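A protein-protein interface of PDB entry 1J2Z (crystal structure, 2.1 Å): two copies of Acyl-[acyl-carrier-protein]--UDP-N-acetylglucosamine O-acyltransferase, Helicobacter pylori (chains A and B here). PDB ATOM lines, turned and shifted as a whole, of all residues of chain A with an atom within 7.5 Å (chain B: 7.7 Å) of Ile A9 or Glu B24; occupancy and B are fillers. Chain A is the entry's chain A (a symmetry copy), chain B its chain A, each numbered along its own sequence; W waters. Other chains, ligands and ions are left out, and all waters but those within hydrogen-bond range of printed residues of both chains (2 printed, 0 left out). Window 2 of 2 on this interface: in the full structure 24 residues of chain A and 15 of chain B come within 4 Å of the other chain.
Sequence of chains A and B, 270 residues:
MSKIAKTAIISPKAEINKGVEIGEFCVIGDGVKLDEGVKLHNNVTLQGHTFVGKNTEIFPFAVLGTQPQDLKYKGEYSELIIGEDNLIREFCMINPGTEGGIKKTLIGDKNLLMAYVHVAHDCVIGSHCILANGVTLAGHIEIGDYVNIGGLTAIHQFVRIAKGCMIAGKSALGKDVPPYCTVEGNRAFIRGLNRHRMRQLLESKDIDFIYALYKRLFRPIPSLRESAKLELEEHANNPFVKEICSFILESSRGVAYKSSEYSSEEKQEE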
ATOM      1  N   ILE A   4     -33.403  17.676  30.651  1.00  0.00           N
ATOM      2  CA  ILE A   4     -32.465  18.675  30.168  1.00  0.00           C
ATOM      3  C   ILE A   4     -33.036  20.059  30.464  1.00  0.00           C
ATOM      4  O   ILE A   4     -34.073  20.435  29.917  1.00  0.00           O
ATOM      5  CB  ILE A   4     -32.248  18.531  28.654  1.00  0.00           C
ATOM      6  CG1 ILE A   4     -31.617  17.167  28.359  1.00  0.00           C
ATOM      7  CG2 ILE A   4     -31.372  19.670  28.138  1.00  0.00           C
ATOM      8  CD1 ILE A   4     -31.466  16.862  26.887  1.00  0.00           C
ATOM      9  N   ALA A   5     -32.361  20.805  31.336  1.00  0.00           N
ATOM     10  CA  ALA A   5     -32.809  22.145  31.703  1.00  0.00           C
ATOM     11  C   ALA A   5     -32.963  23.041  30.473  1.00  0.00           C
ATOM     12  O   ALA A   5     -32.100  23.067  29.593  1.00  0.00           O
ATOM     13  CB  ALA A   5     -31.828  22.771  32.688  1.00  0.00           C
ATOM     14  N   LYS A   6     -34.068  23.779  30.425  1.00  0.00           N
ATOM     15  CA  LYS A   6     -34.351  24.673  29.309  1.00  0.00           C
ATOM     16  C   LYS A   6     -33.360  25.833  29.221  1.00  0.00           C
ATOM     17  O   LYS A   6     -33.129  26.375  28.142  1.00  0.00           O
ATOM     18  CB  LYS A   6     -35.770  25.227  29.438  1.00  0.00           C
ATOM     19  CG  LYS A   6     -36.228  26.050  28.249  1.00  0.00           C
ATOM     20  CD  LYS A   6     -37.694  26.440  28.391  1.00  0.00           C
ATOM     21  CE  LYS A   6     -38.586  25.208  28.548  1.00  0.00           C
ATOM     22  NZ  LYS A   6     -38.465  24.267  27.397  1.00  0.00           N
ATOM     23  N   THR A   7     -32.786  26.215  30.357  1.00  0.00           N
ATOM     24  CA  THR A   7     -31.828  27.316  30.393  1.00  0.00           C
ATOM     25  C   THR A   7     -30.445  26.914  29.882  1.00  0.00           C
ATOM     26  O   THR A   7     -29.619  27.773  29.578  1.00  0.00           O
ATOM     27  CB  THR A   7     -31.649  27.858  31.817  1.00  0.00           C
ATOM     28  OG1 THR A   7     -31.239  26.789  32.673  1.00  0.00           O
ATOM     29  CG2 THR A   7     -32.955  28.465  32.335  1.00  0.00           C
ATOM     30  N   ALA A   8     -30.184  25.614  29.811  1.00  0.00           N
ATOM     31  CA  ALA A   8     -28.889  25.134  29.335  1.00  0.00           C
ATOM     32  C   ALA A   8     -28.670  25.517  27.872  1.00  0.00           C
ATOM     33  O   ALA A   8     -29.613  25.522  27.081  1.00  0.00           O
ATOM     34  CB  ALA A   8     -28.803  23.612  29.495  1.00  0.00           C
ATOM     35  N   ILE A   9     -27.429  25.858  27.526  1.00  0.00           N
ATOM     36  CA  ILE A   9     -27.082  26.219  26.153  1.00  0.00           C
ATOM     37  C   ILE A   9     -26.372  25.013  25.553  1.00  0.00           C
ATOM     38  O   ILE A   9     -25.274  24.648  25.979  1.00  0.00           O
ATOM     39  CB  ILE A   9     -26.135  27.433  26.093  1.00  0.00           C
ATOM     40  CG1 ILE A   9     -26.802  28.656  26.732  1.00  0.00           C
ATOM     41  CG2 ILE A   9     -25.776  27.741  24.628  1.00  0.00           C
ATOM     42  CD1 ILE A   9     -28.101  29.090  26.046  1.00  0.00           C
ATOM     43  N   ILE A  10     -27.005  24.403  24.561  1.00  0.00           N
ATOM     44  CA  ILE A  10     -26.474  23.202  23.932  1.00  0.00           C
ATOM     45  C   ILE A  10     -26.374  23.344  22.418  1.00  0.00           C
ATOM     46  O   ILE A  10     -27.380  23.517  21.735  1.00  0.00           O
ATOM     47  CB  ILE A  10     -27.385  22.001  24.256  1.00  0.00           C
ATOM     48  CG1 ILE A  10     -27.581  21.899  25.773  1.00  0.00           C
ATOM     49  CG2 ILE A  10     -26.785  20.712  23.696  1.00  0.00           C
ATOM     50  CD1 ILE A  10     -28.627  20.885  26.177  1.00  0.00           C
ATOM     51  N   SER A  11     -25.157  23.272  21.897  1.00  0.00           N
ATOM     52  CA  SER A  11     -24.943  23.383  20.459  1.00  0.00           C
ATOM     53  C   SER A  11     -25.723  22.312  19.716  1.00  0.00           C
ATOM     54  O   SER A  11     -25.772  21.158  20.138  1.00  0.00           O
ATOM     55  CB  SER A  11     -23.465  23.220  20.121  1.00  0.00           C
ATOM     56  OG  SER A  11     -23.305  23.015  18.728  1.00  0.00           O
ATOM     57  N   PRO A  12     -26.359  22.684  18.600  1.00  0.00           N
ATOM     58  CA  PRO A  12     -27.112  21.670  17.860  1.00  0.00           C
ATOM     59  C   PRO A  12     -26.182  20.599  17.281  1.00  0.00           C
ATOM     60  O   PRO A  12     -26.627  19.521  16.911  1.00  0.00           O
ATOM     61  CB  PRO A  12     -27.835  22.488  16.787  1.00  0.00           C
ATOM     62  CG  PRO A  12     -26.936  23.696  16.604  1.00  0.00           C
ATOM     63  CD  PRO A  12     -26.564  24.024  18.029  1.00  0.00           C
ATOM     64  N   ILE A  22     -29.100  17.155  32.171  1.00  0.00           N
ATOM     65  CA  ILE A  22     -28.312  18.376  32.072  1.00  0.00           C
ATOM     66  C   ILE A  22     -28.951  19.439  32.960  1.00  0.00           C
ATOM     67  O   ILE A  22     -30.103  19.819  32.757  1.00  0.00           O
ATOM     68  CB  ILE A  22     -28.247  18.858  30.601  1.00  0.00           C
ATOM     69  CG1 ILE A  22     -27.556  17.790  29.745  1.00  0.00           C
ATOM     70  CG2 ILE A  22     -27.501  20.179  30.507  1.00  0.00           C
ATOM     71  CD1 ILE A  22     -27.476  18.126  28.265  1.00  0.00           C
ATOM     72  N   GLY A  23     -28.194  19.906  33.950  1.00  0.00           N
ATOM     73  CA  GLY A  23     -28.710  20.900  34.875  1.00  0.00           C
ATOM     74  C   GLY A  23     -28.832  22.295  34.304  1.00  0.00           C
ATOM     75  O   GLY A  23     -28.490  22.534  33.149  1.00  0.00           O
ATOM     76  N   GLU A  24     -29.313  23.222  35.129  1.00  0.00           N
ATOM     77  CA  GLU A  24     -29.502  24.613  34.722  1.00  0.00           C
ATOM     78  C   GLU A  24     -28.208  25.301  34.285  1.00  0.00           C
ATOM     79  O   GLU A  24     -27.149  25.095  34.873  1.00  0.00           O
ATOM     80  CB  GLU A  24     -30.101  25.426  35.878  1.00  0.00           C
ATOM     81  CG  GLU A  24     -31.327  24.814  36.525  1.00  0.00           C
ATOM     82  CD  GLU A  24     -32.585  25.022  35.717  1.00  0.00           C
ATOM     83  OE1 GLU A  24     -33.630  24.474  36.114  1.00  0.00           O
ATOM     84  OE2 GLU A  24     -32.533  25.740  34.691  1.00  0.00           O
ATOM     85  N   PHE A  25     -28.316  26.128  33.252  1.00  0.00           N
ATOM     86  CA  PHE A  25     -27.195  26.910  32.742  1.00  0.00           C
ATOM     87  C   PHE A  25     -25.946  26.174  32.261  1.00  0.00           C
ATOM     88  O   PHE A  25     -24.871  26.765  32.218  1.00  0.00           O
ATOM     89  CB  PHE A  25     -26.784  27.950  33.797  1.00  0.00           C
ATOM     90  CG  PHE A  25     -27.935  28.780  34.311  1.00  0.00           C
ATOM     91  CD1 PHE A  25     -28.219  28.829  35.672  1.00  0.00           C
ATOM     92  CD2 PHE A  25     -28.751  29.486  33.430  1.00  0.00           C
ATOM     93  CE1 PHE A  25     -29.303  29.567  36.158  1.00  0.00           C
ATOM     94  CE2 PHE A  25     -29.840  30.230  33.898  1.00  0.00           C
ATOM     95  CZ  PHE A  25     -30.117  30.269  35.267  1.00  0.00           C
ATOM     96  N   CYS A  26     -26.050  24.898  31.909  1.00  0.00           N
ATOM     97  CA  CYS A  26     -24.857  24.218  31.410  1.00  0.00           C
ATOM     98  C   CYS A  26     -24.524  24.825  30.053  1.00  0.00           C
ATOM     99  O   CYS A  26     -25.414  25.314  29.358  1.00  0.00           O
ATOM    100  CB  CYS A  26     -25.093  22.714  31.249  1.00  0.00           C
ATOM    101  SG  CYS A  26     -24.986  21.751  32.782  1.00  0.00           S
ATOM    102  N   VAL A  27     -23.246  24.817  29.687  1.00  0.00           N
ATOM    103  CA  VAL A  27     -22.810  25.339  28.392  1.00  0.00           C
ATOM    104  C   VAL A  27     -22.103  24.190  27.686  1.00  0.00           C
ATOM    105  O   VAL A  27     -21.058  23.718  28.141  1.00  0.00           O
ATOM    106  CB  VAL A  27     -21.843  26.529  28.545  1.00  0.00           C
ATOM    107  CG1 VAL A  27     -21.408  27.030  27.163  1.00  0.00           C
ATOM    108  CG2 VAL A  27     -22.530  27.651  29.311  1.00  0.00           C
ATOM    109  N   ILE A  28     -22.693  23.739  26.582  1.00  0.00           N
ATOM    110  CA  ILE A  28     -22.171  22.611  25.822  1.00  0.00           C
ATOM    111  C   ILE A  28     -21.828  22.983  24.380  1.00  0.00           C
ATOM    112  O   ILE A  28     -22.713  23.309  23.588  1.00  0.00           O
ATOM    113  CB  ILE A  28     -23.205  21.462  25.862  1.00  0.00           C
ATOM    114  CG1 ILE A  28     -23.468  21.093  27.326  1.00  0.00           C
ATOM    115  CG2 ILE A  28     -22.715  20.260  25.055  1.00  0.00           C
ATOM    116  CD1 ILE A  28     -24.515  20.024  27.525  1.00  0.00           C
ATOM    117  N   GLY A  29     -20.534  22.920  24.065  1.00  0.00           N
ATOM    118  CA  GLY A  29     -20.031  23.267  22.742  1.00  0.00           C
ATOM    119  C   GLY A  29     -20.369  22.313  21.608  1.00  0.00           C
ATOM    120  O   GLY A  29     -20.897  21.219  21.828  1.00  0.00           O
ATOM    121  N   VAL A  44     -22.267  23.307  34.247  1.00  0.00           N
ATOM    122  CA  VAL A  44     -21.083  22.567  33.833  1.00  0.00           C
ATOM    123  C   VAL A  44     -20.708  23.124  32.455  1.00  0.00           C
ATOM    124  O   VAL A  44     -21.582  23.369  31.619  1.00  0.00           O
ATOM    125  CB  VAL A  44     -21.353  21.048  33.704  1.00  0.00           C
ATOM    126  CG1 VAL A  44     -20.159  20.361  33.043  1.00  0.00           C
ATOM    127  CG2 VAL A  44     -21.604  20.438  35.081  1.00  0.00           C
ATOM    128  N   LEU A  46     -18.699  22.407  29.012  1.00  0.00           N
ATOM    129  CA  LEU A  46     -18.046  21.397  28.191  1.00  0.00           C
ATOM    130  C   LEU A  46     -17.737  22.015  26.829  1.00  0.00           C
ATOM    131  O   LEU A  46     -18.647  22.379  26.087  1.00  0.00           O
ATOM    132  CB  LEU A  46     -18.968  20.183  28.027  1.00  0.00           C
ATOM    133  CG  LEU A  46     -19.471  19.537  29.322  1.00  0.00           C
ATOM    134  CD1 LEU A  46     -20.387  18.361  29.000  1.00  0.00           C
ATOM    135  CD2 LEU A  46     -18.285  19.069  30.148  1.00  0.00           C
ATOM    136  N   GLN A  47     -16.452  22.143  26.514  1.00  0.00           N
ATOM    137  CA  GLN A  47     -16.010  22.724  25.250  1.00  0.00           C
ATOM    138  C   GLN A  47     -15.078  21.758  24.510  1.00  0.00           C
ATOM    139  O   GLN A  47     -14.776  20.671  24.999  1.00  0.00           O
ATOM    140  CB  GLN A  47     -15.249  24.032  25.507  1.00  0.00           C
ATOM    141  CG  GLN A  47     -16.006  25.098  26.301  1.00  0.00           C
ATOM    142  CD  GLN A  47     -17.100  25.780  25.494  1.00  0.00           C
ATOM    143  OE1 GLN A  47     -18.206  25.260  25.354  1.00  0.00           O
ATOM    144  NE2 GLN A  47     -16.788  26.948  24.951  1.00  0.00           N
ATOM    145  N   LYS B   3     -19.142  38.745  18.844  1.00  0.00           N
ATOM    146  CA  LYS B   3     -20.488  38.368  19.245  1.00  0.00           C
ATOM    147  C   LYS B   3     -20.717  38.434  20.751  1.00  0.00           C
ATOM    148  O   LYS B   3     -19.880  38.003  21.545  1.00  0.00           O
ATOM    149  CB  LYS B   3     -20.811  36.960  18.749  1.00  0.00           C
ATOM    150  CG  LYS B   3     -22.229  36.513  19.062  1.00  0.00           C
ATOM    151  CD  LYS B   3     -23.246  37.514  18.522  1.00  0.00           C
ATOM    152  CE  LYS B   3     -24.656  36.981  18.673  1.00  0.00           C
ATOM    153  NZ  LYS B   3     -24.779  35.669  17.988  1.00  0.00           N
ATOM    154  N   ILE B   4     -21.866  38.982  21.129  1.00  0.00           N
ATOM    155  CA  ILE B   4     -22.250  39.112  22.524  1.00  0.00           C
ATOM    156  C   ILE B   4     -23.454  38.209  22.781  1.00  0.00           C
ATOM    157  O   ILE B   4     -24.530  38.430  22.225  1.00  0.00           O
ATOM    158  CB  ILE B   4     -22.630  40.565  22.852  1.00  0.00           C
ATOM    159  CG1 ILE B   4     -21.408  41.466  22.654  1.00  0.00           C
ATOM    160  CG2 ILE B   4     -23.164  40.659  24.278  1.00  0.00           C
ATOM    161  CD1 ILE B   4     -21.692  42.938  22.831  1.00  0.00           C
ATOM    162  N   ALA B   5     -23.262  37.189  23.615  1.00  0.00           N
ATOM    163  CA  ALA B   5     -24.335  36.253  23.938  1.00  0.00           C
ATOM    164  C   ALA B   5     -25.561  36.977  24.497  1.00  0.00           C
ATOM    165  O   ALA B   5     -25.444  37.859  25.350  1.00  0.00           O
ATOM    166  CB  ALA B   5     -23.839  35.215  24.938  1.00  0.00           C
ATOM    167  N   LYS B   6     -26.736  36.591  24.010  1.00  0.00           N
ATOM    168  CA  LYS B   6     -27.988  37.198  24.444  1.00  0.00           C
ATOM    169  C   LYS B   6     -28.300  36.911  25.912  1.00  0.00           C
ATOM    170  O   LYS B   6     -28.993  37.688  26.566  1.00  0.00           O
ATOM    171  CB  LYS B   6     -29.138  36.692  23.573  1.00  0.00           C
ATOM    172  CG  LYS B   6     -30.466  37.376  23.836  1.00  0.00           C
ATOM    173  CD  LYS B   6     -31.519  36.921  22.832  1.00  0.00           C
ATOM    174  CE  LYS B   6     -31.071  37.186  21.395  1.00  0.00           C
ATOM    175  NZ  LYS B   6     -30.784  38.629  21.145  1.00  0.00           N
ATOM    176  N   THR B   7     -27.798  35.790  26.422  1.00  0.00           N
ATOM    177  CA  THR B   7     -28.037  35.413  27.812  1.00  0.00           C
ATOM    178  C   THR B   7     -27.170  36.196  28.796  1.00  0.00           C
ATOM    179  O   THR B   7     -27.445  36.210  29.994  1.00  0.00           O
ATOM    180  CB  THR B   7     -27.757  33.922  28.043  1.00  0.00           C
ATOM    181  OG1 THR B   7     -26.411  33.635  27.654  1.00  0.00           O
ATOM    182  CG2 THR B   7     -28.724  33.056  27.234  1.00  0.00           C
ATOM    183  N   ALA B   8     -26.114  36.827  28.298  1.00  0.00           N
ATOM    184  CA  ALA B   8     -25.226  37.602  29.162  1.00  0.00           C
ATOM    185  C   ALA B   8     -25.965  38.790  29.776  1.00  0.00           C
ATOM    186  O   ALA B   8     -26.818  39.396  29.128  1.00  0.00           O
ATOM    187  CB  ALA B   8     -24.016  38.095  28.363  1.00  0.00           C
ATOM    188  N   ILE B   9     -25.649  39.103  31.032  1.00  0.00           N
ATOM    189  CA  ILE B   9     -26.264  40.233  31.725  1.00  0.00           C
ATOM    190  C   ILE B   9     -25.232  41.353  31.726  1.00  0.00           C
ATOM    191  O   ILE B   9     -24.178  41.243  32.357  1.00  0.00           O
ATOM    192  CB  ILE B   9     -26.629  39.893  33.183  1.00  0.00           C
ATOM    193  CG1 ILE B   9     -27.632  38.736  33.219  1.00  0.00           C
ATOM    194  CG2 ILE B   9     -27.235  41.130  33.869  1.00  0.00           C
ATOM    195  CD1 ILE B   9     -28.953  39.029  32.503  1.00  0.00           C
ATOM    196  N   ILE B  22     -18.451  38.310  24.127  1.00  0.00           N
ATOM    197  CA  ILE B  22     -18.928  37.985  25.464  1.00  0.00           C
ATOM    198  C   ILE B  22     -19.700  36.671  25.399  1.00  0.00           C
ATOM    199  O   ILE B  22     -20.706  36.567  24.698  1.00  0.00           O
ATOM    200  CB  ILE B  22     -19.828  39.122  26.008  1.00  0.00           C
ATOM    201  CG1 ILE B  22     -19.010  40.414  26.110  1.00  0.00           C
ATOM    202  CG2 ILE B  22     -20.398  38.746  27.367  1.00  0.00           C
ATOM    203  CD1 ILE B  22     -19.799  41.623  26.586  1.00  0.00           C
ATOM    204  N   GLY B  23     -19.213  35.669  26.126  1.00  0.00           N
ATOM    205  CA  GLY B  23     -19.851  34.364  26.116  1.00  0.00           C
ATOM    206  C   GLY B  23     -21.155  34.290  26.878  1.00  0.00           C
ATOM    207  O   GLY B  23     -21.597  35.274  27.466  1.00  0.00           O
ATOM    208  N   GLU B  24     -21.766  33.108  26.875  1.00  0.00           N
ATOM    209  CA  GLU B  24     -23.039  32.879  27.555  1.00  0.00           C
ATOM    210  C   GLU B  24     -22.980  33.135  29.061  1.00  0.00           C
ATOM    211  O   GLU B  24     -21.998  32.809  29.724  1.00  0.00           O
ATOM    212  CB  GLU B  24     -23.502  31.431  27.342  1.00  0.00           C
ATOM    213  CG  GLU B  24     -23.492  30.961  25.901  1.00  0.00           C
ATOM    214  CD  GLU B  24     -24.678  31.463  25.111  1.00  0.00           C
ATOM    215  OE1 GLU B  24     -24.713  31.212  23.892  1.00  0.00           O
ATOM    216  OE2 GLU B  24     -25.576  32.100  25.707  1.00  0.00           O
ATOM    217  N   PHE B  25     -24.051  33.716  29.588  1.00  0.00           N
ATOM    218  CA  PHE B  25     -24.187  33.980  31.017  1.00  0.00           C
ATOM    219  C   PHE B  25     -23.143  34.860  31.702  1.00  0.00           C
ATOM    220  O   PHE B  25     -22.979  34.776  32.916  1.00  0.00           O
ATOM    221  CB  PHE B  25     -24.283  32.644  31.771  1.00  0.00           C
ATOM    222  CG  PHE B  25     -25.326  31.707  31.213  1.00  0.00           C
ATOM    223  CD1 PHE B  25     -24.977  30.425  30.801  1.00  0.00           C
ATOM    224  CD2 PHE B  25     -26.649  32.120  31.071  1.00  0.00           C
ATOM    225  CE1 PHE B  25     -25.928  29.558  30.252  1.00  0.00           C
ATOM    226  CE2 PHE B  25     -27.614  31.266  30.523  1.00  0.00           C
ATOM    227  CZ  PHE B  25     -27.251  29.981  30.112  1.00  0.00           C
ATOM    228  N   CYS B  26     -22.422  35.695  30.962  1.00  0.00           N
ATOM    229  CA  CYS B  26     -21.458  36.560  31.635  1.00  0.00           C
ATOM    230  C   CYS B  26     -22.251  37.574  32.450  1.00  0.00           C
ATOM    231  O   CYS B  26     -23.385  37.899  32.100  1.00  0.00           O
ATOM    232  CB  CYS B  26     -20.570  37.300  30.631  1.00  0.00           C
ATOM    233  SG  CYS B  26     -19.201  36.325  29.952  1.00  0.00           S
ATOM    234  N   VAL B  27     -21.670  38.052  33.547  1.00  0.00           N
ATOM    235  CA  VAL B  27     -22.320  39.056  34.389  1.00  0.00           C
ATOM    236  C   VAL B  27     -21.373  40.248  34.436  1.00  0.00           C
ATOM    237  O   VAL B  27     -20.260  40.150  34.959  1.00  0.00           O
ATOM    238  CB  VAL B  27     -22.571  38.536  35.818  1.00  0.00           C
ATOM    239  CG1 VAL B  27     -23.240  39.627  36.662  1.00  0.00           C
ATOM    240  CG2 VAL B  27     -23.461  37.302  35.763  1.00  0.00           C
ATOM    241  N   LEU B  40     -14.446  37.374  26.345  1.00  0.00           N
ATOM    242  CA  LEU B  40     -14.887  36.767  27.585  1.00  0.00           C
ATOM    243  C   LEU B  40     -15.572  35.468  27.226  1.00  0.00           C
ATOM    244  O   LEU B  40     -16.493  35.457  26.411  1.00  0.00           O
ATOM    245  CB  LEU B  40     -15.898  37.661  28.307  1.00  0.00           C
ATOM    246  CG  LEU B  40     -15.493  39.085  28.679  1.00  0.00           C
ATOM    247  CD1 LEU B  40     -16.628  39.727  29.463  1.00  0.00           C
ATOM    248  CD2 LEU B  40     -14.217  39.066  29.502  1.00  0.00           C
ATOM    249  N   HIS B  41     -15.126  34.367  27.818  1.00  0.00           N
ATOM    250  CA  HIS B  41     -15.778  33.096  27.552  1.00  0.00           C
ATOM    251  C   HIS B  41     -17.081  33.113  28.329  1.00  0.00           C
ATOM    252  O   HIS B  41     -17.459  34.140  28.888  1.00  0.00           O
ATOM    253  CB  HIS B  41     -14.891  31.939  28.003  1.00  0.00           C
ATOM    254  CG  HIS B  41     -13.652  31.787  27.175  1.00  0.00           C
ATOM    255  ND1 HIS B  41     -13.316  30.608  26.546  1.00  0.00           N
ATOM    256  CD2 HIS B  41     -12.684  32.675  26.850  1.00  0.00           C
ATOM    257  CE1 HIS B  41     -12.195  30.777  25.868  1.00  0.00           C
ATOM    258  NE2 HIS B  41     -11.791  32.024  26.037  1.00  0.00           N
ATOM    259  N   ASN B  42     -17.780  31.990  28.363  1.00  0.00           N
ATOM    260  CA  ASN B  42     -19.033  31.940  29.100  1.00  0.00           C
ATOM    261  C   ASN B  42     -18.787  32.098  30.599  1.00  0.00           C
ATOM    262  O   ASN B  42     -17.717  31.764  31.103  1.00  0.00           O
ATOM    263  CB  ASN B  42     -19.733  30.601  28.854  1.00  0.00           C
ATOM    264  CG  ASN B  42     -18.969  29.427  29.450  1.00  0.00           C
ATOM    265  OD1 ASN B  42     -19.254  28.980  30.569  1.00  0.00           O
ATOM    266  ND2 ASN B  42     -17.983  28.935  28.715  1.00  0.00           N
ATOM    267  N   ASN B  43     -19.783  32.633  31.295  1.00  0.00           N
ATOM    268  CA  ASN B  43     -19.733  32.768  32.746  1.00  0.00           C
ATOM    269  C   ASN B  43     -18.583  33.535  33.395  1.00  0.00           C
ATOM    270  O   ASN B  43     -18.034  33.093  34.409  1.00  0.00           O
ATOM    271  CB  ASN B  43     -19.813  31.373  33.368  1.00  0.00           C
ATOM    272  CG  ASN B  43     -21.161  30.712  33.142  1.00  0.00           C
ATOM    273  OD1 ASN B  43     -22.150  31.061  33.787  1.00  0.00           O
ATOM    274  ND2 ASN B  43     -21.208  29.766  32.219  1.00  0.00           N
ATOM    275  N   VAL B  44     -18.201  34.666  32.816  1.00  0.00           N
ATOM    276  CA  VAL B  44     -17.165  35.479  33.436  1.00  0.00           C
ATOM    277  C   VAL B  44     -17.907  36.536  34.262  1.00  0.00           C
ATOM    278  O   VAL B  44     -18.912  37.093  33.809  1.00  0.00           O
ATOM    279  CB  VAL B  44     -16.273  36.193  32.391  1.00  0.00           C
ATOM    280  CG1 VAL B  44     -15.368  37.208  33.086  1.00  0.00           C
ATOM    281  CG2 VAL B  44     -15.423  35.171  31.638  1.00  0.00           C
ATOM    282  N   PHE B  61     -15.794  31.113  34.521  1.00  0.00           N
ATOM    283  CA  PHE B  61     -15.834  31.191  35.970  1.00  0.00           C
ATOM    284  C   PHE B  61     -14.760  32.021  36.653  1.00  0.00           C
ATOM    285  O   PHE B  61     -14.470  31.818  37.833  1.00  0.00           O
ATOM    286  CB  PHE B  61     -15.857  29.773  36.541  1.00  0.00           C
ATOM    287  CG  PHE B  61     -16.965  28.914  35.969  1.00  0.00           C
ATOM    288  CD1 PHE B  61     -16.722  27.597  35.593  1.00  0.00           C
ATOM    289  CD2 PHE B  61     -18.248  29.430  35.802  1.00  0.00           C
ATOM    290  CE1 PHE B  61     -17.742  26.805  35.057  1.00  0.00           C
ATOM    291  CE2 PHE B  61     -19.277  28.648  35.267  1.00  0.00           C
ATOM    292  CZ  PHE B  61     -19.023  27.335  34.893  1.00  0.00           C
HETATM  293  O   HOH W   1     -22.313  27.483  33.235  1.00  0.00           O
HETATM  294  O   HOH W   2     -14.897  28.188  26.684  1.00  0.00           O
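Of the printed residues of chain B, Thr A7 touches Phe B25.
No residue of chain B comes within 4 Å of Ala A8.
Ile A9 touches just these residues of chain B: Glu B24 and Phe B25.
Of the printed residues of chain B, Val A27 touches Phe B25, Asn B42 and Asn B43.
Of chain A, only Ile A9 comes within 4 Å of Glu B24.
Cys B26 touches none of the printed residues of chain A.
Of the printed residues of chain A, Asn B42 touches Val A27.
The nearest residue of chain B that does not touch Ile A9 is Thr B7 (4.2 Å).
The nearest printed residue of chain A that does not touch Asn B43 is Phe A25 (4.7 Å).
Of the 20 printed residues of chain A, 4 touch a printed residue of chain B.
Hydrophobic or aromatic side chains of chain A that line the printed part of chain B: Ile A9, Phe A25 and Val A27.
Of the 19 printed residues of chain B, 4 touch a printed residue of chain A.
Printed residues of chain B that touch a printed residue of chain A: Glu B24, Phe B25, Asn B42 and Asn B43.
Hydrophobic or aromatic side chains of chain B that line the printed part of chain A: Phe B25.
Among the printed residues, 7 pairs touch across the chains.
Among the printed residues, no Asp or Glu carboxylate lies within 4 Å of a Lys or Arg side-chain nitrogen of the other chain.
Water W1 bridges the side-chain amide nitrogen of Asn B43 (2.7 Å) and the backbone carbonyl oxygen of Phe A25 (2.8 Å).
Water W2 bridges NE2 of Gln A47 and ND1 of His B41.
Thr A7 touches Phe B25, but with the chains exchanged Phe A25 does not touch Thr B7 (7.0 Å).
Ile A9 touches Phe B25, but with the chains exchanged Phe A25 does not touch Ile B9 (8.8 Å).
Phe A25 touches its own counterpart, Phe B25.
Val A27 touches Phe B25, but with the chains exchanged Phe A25 does not touch Val B27 (9.7 Å).
Positions printed for both chains: 4, 5, 6, 7, 8, 9, 22, 23, 24, 25, 26, 27 and 44.
Of the 7 pairs that touch across the chains among the printed residues, 1 has its exchanged pair printed and touching as well.
Thr A7 touches Phe B25 (O to CZ, 3.3 Å).
CG2 of Ile A9 touches OE1 of Glu B24, 3.7 Å away.
Phe B25 touches Ile A9.
O of Phe A25 touches CE1 of Phe B25, 3.6 Å away.
Val A27 touches Phe B25 (CG2 to CD1, 3.99 Å).
Val A27 touches Asn B42 (CG2 to OD1, 3.8 Å).
Val A27 touches Asn B43 (CG2 to ND2, 3.8 Å).
O of Asn B43 sits at hydrogen-bond distance from N of Phe B61 (3.0 Å).
The side-chain hydroxyl (OG1) of Thr A7 sits at hydrogen-bond distance from the side-chain carboxylate (OE2) of Glu A24 (2.6 Å).
The side-chain hydroxyl of Thr A7 is in hydrogen-bond range of the backbone NH of Phe A25 (3.1 Å).
The backbone NH of Ile A9 is in hydrogen-bond range of the backbone carbonyl oxygen of Cys A26 (2.8 Å).
The backbone carbonyl oxygen (O) of Ile A9 is in hydrogen-bond range of the backbone NH (N) of Ile A28 (2.8 Å).
The side-chain hydroxyl of Thr B7 sits at hydrogen-bond distance from the backbone NH of Phe B25, 3.1 Å away.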
